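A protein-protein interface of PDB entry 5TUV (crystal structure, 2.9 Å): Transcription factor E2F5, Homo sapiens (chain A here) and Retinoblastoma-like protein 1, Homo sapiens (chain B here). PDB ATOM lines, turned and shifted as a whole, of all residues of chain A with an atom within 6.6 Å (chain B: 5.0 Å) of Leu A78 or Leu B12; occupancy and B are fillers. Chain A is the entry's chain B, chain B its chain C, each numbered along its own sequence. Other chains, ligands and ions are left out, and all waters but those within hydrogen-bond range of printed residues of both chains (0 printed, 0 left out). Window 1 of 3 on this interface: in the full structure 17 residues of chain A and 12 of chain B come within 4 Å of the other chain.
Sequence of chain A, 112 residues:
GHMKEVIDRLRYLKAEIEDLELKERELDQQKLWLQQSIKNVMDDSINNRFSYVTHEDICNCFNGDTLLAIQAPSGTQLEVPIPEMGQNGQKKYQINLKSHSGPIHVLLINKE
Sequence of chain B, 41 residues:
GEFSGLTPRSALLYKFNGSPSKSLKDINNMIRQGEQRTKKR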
ATOM      1  N   ILE A  70       2.791 -30.630 -22.281  1.00  0.00           N
ATOM      2  CA  ILE A  70       3.942 -30.603 -21.392  1.00  0.00           C
ATOM      3  C   ILE A  70       3.582 -29.899 -20.095  1.00  0.00           C
ATOM      4  O   ILE A  70       3.145 -28.751 -20.101  1.00  0.00           O
ATOM      5  CB  ILE A  70       5.146 -29.891 -22.024  1.00  0.00           C
ATOM      6  CG1 ILE A  70       5.494 -30.506 -23.381  1.00  0.00           C
ATOM      7  CG2 ILE A  70       6.341 -29.936 -21.082  1.00  0.00           C
ATOM      8  CD1 ILE A  70       6.695 -29.865 -24.049  1.00  0.00           C
ATOM      9  N   THR A  76       9.273 -22.518 -14.574  1.00  0.00           N
ATOM     10  CA  THR A  76       9.994 -23.316 -15.556  1.00  0.00           C
ATOM     11  C   THR A  76      10.231 -22.450 -16.785  1.00  0.00           C
ATOM     12  O   THR A  76       9.296 -21.844 -17.309  1.00  0.00           O
ATOM     13  CB  THR A  76       9.225 -24.591 -15.946  1.00  0.00           C
ATOM     14  OG1 THR A  76       8.937 -25.358 -14.769  1.00  0.00           O
ATOM     15  CG2 THR A  76      10.043 -25.438 -16.907  1.00  0.00           C
ATOM     16  N   GLN A  77      11.474 -22.387 -17.247  1.00  0.00           N
ATOM     17  CA  GLN A  77      11.790 -21.526 -18.377  1.00  0.00           C
ATOM     18  C   GLN A  77      11.800 -22.293 -19.691  1.00  0.00           C
ATOM     19  O   GLN A  77      12.323 -23.403 -19.781  1.00  0.00           O
ATOM     20  CB  GLN A  77      13.137 -20.832 -18.172  1.00  0.00           C
ATOM     21  CG  GLN A  77      13.176 -19.420 -18.740  1.00  0.00           C
ATOM     22  CD  GLN A  77      14.579 -18.954 -19.069  1.00  0.00           C
ATOM     23  OE1 GLN A  77      15.451 -19.756 -19.402  1.00  0.00           O
ATOM     24  NE2 GLN A  77      14.805 -17.648 -18.975  1.00  0.00           N
ATOM     25  N   LEU A  78      11.203 -21.679 -20.705  1.00  0.00           N
ATOM     26  CA  LEU A  78      11.126 -22.250 -22.039  1.00  0.00           C
ATOM     27  C   LEU A  78      11.835 -21.354 -23.046  1.00  0.00           C
ATOM     28  O   LEU A  78      11.483 -20.185 -23.201  1.00  0.00           O
ATOM     29  CB  LEU A  78       9.666 -22.462 -22.444  1.00  0.00           C
ATOM     30  CG  LEU A  78       9.395 -23.065 -23.822  1.00  0.00           C
ATOM     31  CD1 LEU A  78       8.285 -24.089 -23.731  1.00  0.00           C
ATOM     32  CD2 LEU A  78       9.024 -21.977 -24.817  1.00  0.00           C
ATOM     33  N   GLU A  79      12.835 -21.903 -23.725  1.00  0.00           N
ATOM     34  CA  GLU A  79      13.632 -21.122 -24.662  1.00  0.00           C
ATOM     35  C   GLU A  79      13.552 -21.718 -26.064  1.00  0.00           C
ATOM     36  O   GLU A  79      13.869 -22.888 -26.273  1.00  0.00           O
ATOM     37  CB  GLU A  79      15.087 -21.054 -24.195  1.00  0.00           C
ATOM     38  CG  GLU A  79      16.043 -20.444 -25.204  1.00  0.00           C
ATOM     39  CD  GLU A  79      17.468 -20.382 -24.687  1.00  0.00           C
ATOM     40  OE1 GLU A  79      17.669 -20.585 -23.472  1.00  0.00           O
ATOM     41  OE2 GLU A  79      18.387 -20.133 -25.496  1.00  0.00           O
ATOM     42  N   VAL A  80      13.124 -20.900 -27.021  1.00  0.00           N
ATOM     43  CA  VAL A  80      13.017 -21.332 -28.410  1.00  0.00           C
ATOM     44  C   VAL A  80      13.920 -20.509 -29.320  1.00  0.00           C
ATOM     45  O   VAL A  80      13.696 -19.314 -29.508  1.00  0.00           O
ATOM     46  CB  VAL A  80      11.571 -21.233 -28.927  1.00  0.00           C
ATOM     47  CG1 VAL A  80      11.504 -21.652 -30.387  1.00  0.00           C
ATOM     48  CG2 VAL A  80      10.645 -22.089 -28.081  1.00  0.00           C
ATOM     49  N   PRO A  81      14.950 -21.152 -29.887  1.00  0.00           N
ATOM     50  CA  PRO A  81      15.888 -20.464 -30.777  1.00  0.00           C
ATOM     51  C   PRO A  81      15.300 -20.214 -32.161  1.00  0.00           C
ATOM     52  O   PRO A  81      14.261 -20.775 -32.510  1.00  0.00           O
ATOM     53  CB  PRO A  81      17.065 -21.435 -30.855  1.00  0.00           C
ATOM     54  CG  PRO A  81      16.441 -22.767 -30.672  1.00  0.00           C
ATOM     55  CD  PRO A  81      15.306 -22.569 -29.701  1.00  0.00           C
ATOM     56  N   ILE A  82      15.971 -19.369 -32.933  1.00  0.00           N
ATOM     57  CA  ILE A  82      15.549 -19.049 -34.290  1.00  0.00           C
ATOM     58  C   ILE A  82      15.717 -20.239 -35.237  1.00  0.00           C
ATOM     59  O   ILE A  82      16.666 -21.012 -35.118  1.00  0.00           O
ATOM     60  CB  ILE A  82      16.314 -17.808 -34.835  1.00  0.00           C
ATOM     61  CG1 ILE A  82      17.735 -17.705 -34.257  1.00  0.00           C
ATOM     62  CG2 ILE A  82      15.563 -16.536 -34.493  1.00  0.00           C
ATOM     63  CD1 ILE A  82      18.688 -18.831 -34.605  1.00  0.00           C
ATOM     64  N   ILE A  95      12.930 -26.849 -28.731  1.00  0.00           N
ATOM     65  CA  ILE A  95      12.436 -26.207 -27.528  1.00  0.00           C
ATOM     66  C   ILE A  95      13.348 -26.592 -26.375  1.00  0.00           C
ATOM     67  O   ILE A  95      13.506 -27.773 -26.067  1.00  0.00           O
ATOM     68  CB  ILE A  95      10.988 -26.624 -27.206  1.00  0.00           C
ATOM     69  CG1 ILE A  95      10.025 -26.103 -28.274  1.00  0.00           C
ATOM     70  CG2 ILE A  95      10.585 -26.129 -25.826  1.00  0.00           C
ATOM     71  CD1 ILE A  95       8.595 -26.542 -28.067  1.00  0.00           C
ATOM     72  N   ASN A  96      13.958 -25.594 -25.748  1.00  0.00           N
ATOM     73  CA  ASN A  96      14.831 -25.850 -24.612  1.00  0.00           C
ATOM     74  C   ASN A  96      14.099 -25.577 -23.308  1.00  0.00           C
ATOM     75  O   ASN A  96      13.742 -24.440 -23.000  1.00  0.00           O
ATOM     76  CB  ASN A  96      16.103 -25.006 -24.703  1.00  0.00           C
ATOM     77  CG  ASN A  96      16.831 -25.192 -26.018  1.00  0.00           C
ATOM     78  OD1 ASN A  96      16.491 -24.570 -27.024  1.00  0.00           O
ATOM     79  ND2 ASN A  96      17.841 -26.055 -26.019  1.00  0.00           N
ATOM     80  N   LEU A  97      13.881 -26.646 -22.552  1.00  0.00           N
ATOM     81  CA  LEU A  97      13.173 -26.584 -21.282  1.00  0.00           C
ATOM     82  C   LEU A  97      14.121 -26.695 -20.099  1.00  0.00           C
ATOM     83  O   LEU A  97      14.974 -27.582 -20.056  1.00  0.00           O
ATOM     84  CB  LEU A  97      12.114 -27.685 -21.200  1.00  0.00           C
ATOM     85  CG  LEU A  97      10.801 -27.434 -21.937  1.00  0.00           C
ATOM     86  CD1 LEU A  97       9.879 -28.636 -21.800  1.00  0.00           C
ATOM     87  CD2 LEU A  97      10.132 -26.182 -21.400  1.00  0.00           C
ATOM     88  N   LYS A  98      13.978 -25.782 -19.148  1.00  0.00           N
ATOM     89  CA  LYS A  98      14.796 -25.825 -17.947  1.00  0.00           C
ATOM     90  C   LYS A  98      13.900 -25.798 -16.718  1.00  0.00           C
ATOM     91  O   LYS A  98      13.194 -24.822 -16.469  1.00  0.00           O
ATOM     92  CB  LYS A  98      15.782 -24.655 -17.916  1.00  0.00           C
ATOM     93  N   SER B  10      19.434 -14.254 -28.669  1.00  0.00           N
ATOM     94  CA  SER B  10      19.295 -14.953 -29.941  1.00  0.00           C
ATOM     95  C   SER B  10      18.123 -15.928 -29.910  1.00  0.00           C
ATOM     96  O   SER B  10      17.973 -16.764 -30.802  1.00  0.00           O
ATOM     97  CB  SER B  10      20.586 -15.695 -30.289  1.00  0.00           C
ATOM     98  OG  SER B  10      20.453 -16.409 -31.506  1.00  0.00           O
ATOM     99  N   ALA B  11      17.293 -15.814 -28.878  1.00  0.00           N
ATOM    100  CA  ALA B  11      16.143 -16.695 -28.720  1.00  0.00           C
ATOM    101  C   ALA B  11      15.041 -16.025 -27.907  1.00  0.00           C
ATOM    102  O   ALA B  11      15.287 -15.061 -27.184  1.00  0.00           O
ATOM    103  CB  ALA B  11      16.564 -18.001 -28.064  1.00  0.00           C
ATOM    104  N   LEU B  12      13.825 -16.546 -28.031  1.00  0.00           N
ATOM    105  CA  LEU B  12      12.690 -16.033 -27.275  1.00  0.00           C
ATOM    106  C   LEU B  12      12.441 -16.887 -26.037  1.00  0.00           C
ATOM    107  O   LEU B  12      12.607 -18.106 -26.070  1.00  0.00           O
ATOM    108  CB  LEU B  12      11.438 -15.985 -28.153  1.00  0.00           C
ATOM    109  CG  LEU B  12      11.559 -15.141 -29.424  1.00  0.00           C
ATOM    110  CD1 LEU B  12      10.267 -15.179 -30.223  1.00  0.00           C
ATOM    111  CD2 LEU B  12      11.940 -13.708 -29.083  1.00  0.00           C
ATOM    112  N   LEU B  13      12.041 -16.242 -24.946  1.00  0.00           N
ATOM    113  CA  LEU B  13      11.856 -16.935 -23.676  1.00  0.00           C
ATOM    114  C   LEU B  13      10.393 -16.972 -23.247  1.00  0.00           C
ATOM    115  O   LEU B  13       9.637 -16.033 -23.492  1.00  0.00           O
ATOM    116  CB  LEU B  13      12.694 -16.275 -22.575  1.00  0.00           C
ATOM    117  CG  LEU B  13      14.219 -16.228 -22.723  1.00  0.00           C
ATOM    118  CD1 LEU B  13      14.753 -17.531 -23.298  1.00  0.00           C
ATOM    119  CD2 LEU B  13      14.675 -15.032 -23.553  1.00  0.00           C
ATOM    120  N   TYR B  14      10.004 -18.067 -22.602  1.00  0.00           N
ATOM    121  CA  TYR B  14       8.685 -18.176 -21.992  1.00  0.00           C
ATOM    122  C   TYR B  14       8.782 -18.825 -20.616  1.00  0.00           C
ATOM    123  O   TYR B  14       9.573 -19.746 -20.408  1.00  0.00           O
ATOM    124  CB  TYR B  14       7.727 -18.973 -22.880  1.00  0.00           C
ATOM    125  CG  TYR B  14       6.434 -19.323 -22.182  1.00  0.00           C
ATOM    126  CD1 TYR B  14       5.433 -18.376 -22.018  1.00  0.00           C
ATOM    127  CD2 TYR B  14       6.220 -20.598 -21.670  1.00  0.00           C
ATOM    128  CE1 TYR B  14       4.254 -18.688 -21.371  1.00  0.00           C
ATOM    129  CE2 TYR B  14       5.045 -20.919 -21.022  1.00  0.00           C
ATOM    130  CZ  TYR B  14       4.066 -19.961 -20.877  1.00  0.00           C
ATOM    131  OH  TYR B  14       2.895 -20.280 -20.231  1.00  0.00           O
ATOM    132  N   LYS B  15       7.970 -18.344 -19.679  1.00  0.00           N
ATOM    133  CA  LYS B  15       7.973 -18.872 -18.320  1.00  0.00           C
ATOM    134  C   LYS B  15       6.616 -19.457 -17.946  1.00  0.00           C
ATOM    135  O   LYS B  15       5.583 -18.808 -18.112  1.00  0.00           O
ATOM    136  CB  LYS B  15       8.366 -17.778 -17.325  1.00  0.00           C
ATOM    137  CG  LYS B  15       8.520 -18.263 -15.894  1.00  0.00           C
ATOM    138  CD  LYS B  15       8.948 -17.131 -14.975  1.00  0.00           C
ATOM    139  CE  LYS B  15      10.205 -16.447 -15.493  1.00  0.00           C
ATOM    140  NZ  LYS B  15      11.326 -17.409 -15.678  1.00  0.00           N
ATOM    141  N   PHE B  16       6.627 -20.688 -17.443  1.00  0.00           N
ATOM    142  CA  PHE B  16       5.406 -21.354 -17.005  1.00  0.00           C
ATOM    143  C   PHE B  16       4.772 -20.613 -15.834  1.00  0.00           C
ATOM    144  O   PHE B  16       5.402 -20.436 -14.790  1.00  0.00           O
ATOM    145  CB  PHE B  16       5.695 -22.806 -16.609  1.00  0.00           C
ATOM    146  CG  PHE B  16       5.902 -23.730 -17.777  1.00  0.00           C
ATOM    147  CD1 PHE B  16       7.025 -23.617 -18.582  1.00  0.00           C
ATOM    148  CD2 PHE B  16       4.977 -24.720 -18.064  1.00  0.00           C
ATOM    149  CE1 PHE B  16       7.217 -24.469 -19.652  1.00  0.00           C
ATOM    150  CE2 PHE B  16       5.164 -25.575 -19.132  1.00  0.00           C
ATOM    151  CZ  PHE B  16       6.286 -25.449 -19.928  1.00  0.00           C
ATOM    152  N   LEU B  24       4.212 -16.196 -26.341  1.00  0.00           N
ATOM    153  CA  LEU B  24       4.063 -17.391 -27.163  1.00  0.00           C
ATOM    154  C   LEU B  24       3.609 -17.053 -28.579  1.00  0.00           C
ATOM    155  O   LEU B  24       3.920 -17.775 -29.527  1.00  0.00           O
ATOM    156  CB  LEU B  24       3.078 -18.367 -26.519  1.00  0.00           C
ATOM    157  CG  LEU B  24       3.584 -19.100 -25.275  1.00  0.00           C
ATOM    158  CD1 LEU B  24       2.556 -20.110 -24.795  1.00  0.00           C
ATOM    159  CD2 LEU B  24       4.917 -19.778 -25.558  1.00  0.00           C
ATOM    160  N   ASP B  26       4.589 -14.424 -30.240  1.00  0.00           N
ATOM    161  CA  ASP B  26       5.810 -14.004 -30.918  1.00  0.00           C
ATOM    162  C   ASP B  26       6.670 -15.212 -31.269  1.00  0.00           C
ATOM    163  O   ASP B  26       7.336 -15.233 -32.304  1.00  0.00           O
ATOM    164  CB  ASP B  26       6.599 -13.024 -30.048  1.00  0.00           C
ATOM    165  CG  ASP B  26       5.820 -11.759 -29.742  1.00  0.00           C
ATOM    166  OD1 ASP B  26       4.995 -11.350 -30.586  1.00  0.00           O
ATOM    167  OD2 ASP B  26       6.033 -11.175 -28.659  1.00  0.00           O
ATOM    168  N   ILE B  27       6.649 -16.217 -30.399  1.00  0.00           N
ATOM    169  CA  ILE B  27       7.375 -17.456 -30.641  1.00  0.00           C
ATOM    170  C   ILE B  27       6.784 -18.200 -31.836  1.00  0.00           C
ATOM    171  O   ILE B  27       7.510 -18.638 -32.727  1.00  0.00           O
ATOM    172  CB  ILE B  27       7.357 -18.374 -29.402  1.00  0.00           C
ATOM    173  CG1 ILE B  27       8.182 -17.755 -28.272  1.00  0.00           C
ATOM    174  CG2 ILE B  27       7.897 -19.752 -29.748  1.00  0.00           C
ATOM    175  CD1 ILE B  27       8.244 -18.607 -27.021  1.00  0.00           C
ATOM    176  N   MET B  30       7.602 -16.394 -35.057  1.00  0.00           N
ATOM    177  CA  MET B  30       9.012 -16.547 -35.400  1.00  0.00           C
ATOM    178  C   MET B  30       9.272 -17.889 -36.076  1.00  0.00           C
ATOM    179  O   MET B  30       9.983 -17.964 -37.078  1.00  0.00           O
ATOM    180  CB  MET B  30       9.884 -16.413 -34.151  1.00  0.00           C
ATOM    181  CG  MET B  30      11.374 -16.544 -34.419  1.00  0.00           C
ATOM    182  SD  MET B  30      12.329 -16.778 -32.907  1.00  0.00           S
ATOM    183  CE  MET B  30      11.683 -18.348 -32.339  1.00  0.00           C
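The backbone carbonyl oxygen (O) of Thr A76 lies within hydrogen-bond range of the backbone NH (N) of Phe B16, at 2.9 Å. N of Leu A78 sits at hydrogen-bond distance from O of Tyr B14 (2.5 Å). N of Val A80 is in hydrogen-bond range of O of Leu B12.
The backbone NH (N) of Lys A98 is in hydrogen-bond range of the backbone carbonyl oxygen (O) of Gln A77 (3.0 Å). O of Glu A79 lies within hydrogen-bond range of N of Asn A96 (2.8 Å).
Among the printed residues, merely in contact across the chains: Ile A70 with Phe B16, Thr A76 with Tyr B14, Thr A76 with Lys B15, Gln A77 with Tyr B14, Leu A78 with Leu B12, Leu A78 with Leu B13, Glu A79 with Ala B11, Glu A79 with Leu B12, Glu A79 with Leu B13, Val A80 with Ala B11, Val A80 with Ile B27, Val A80 with Met B30, Pro A81 with Ala B11, Pro A81 with Met B30, Ile A82 with Ser B10, Ile A82 with Met B30 and Leu A97 with Phe B16.
Of chain B, only Leu B12, Leu B13 and Tyr B14 come within 4 Å of Leu A78. Leu B12 touches just these residues of chain A: Leu A78 (3.7 Å), Glu A79 (3.5 Å) and Val A80 (3.0 Å). Of the printed residues of chain B, Pro A81 touches Ala B11 and Met B30. Printed residues of chain B within 4 Å of Glu A79: Ala B11, Leu B12 and Leu B13. Of the printed residues of chain A, Phe B16 touches Ile A70 (3.9 Å), Thr A76 (2.9 Å) and Leu A97 (3.8 Å). Leu B24 touches none of the printed residues of chain A. Ile A95 touches none of the printed residues of chain B. The nearest residue of chain B that does not touch Leu A78 is Ile B27 (4.1 Å). The nearest residue of chain A that does not touch Leu B12 is Pro A81 (5.1 Å).
Printed residues of chain A that touch a printed residue of chain B: Ile A70, Thr A76, Gln A77, Leu A78, Glu A79, Val A80, Pro A81, Ile A82 and Leu A97. Hydrophobic or aromatic side chains of chain A that line the printed part of chain B: Leu A78, Val A80, Ile A82 and Leu A97. Of the 11 printed residues of chain B, 9 touch a printed residue of chain A. Hydrophobic or aromatic side chains of chain B within 4 Å of the printed part of chain A: Ala B11, Leu B13, Tyr B14, Phe B16, Ile B27 and Met B30.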
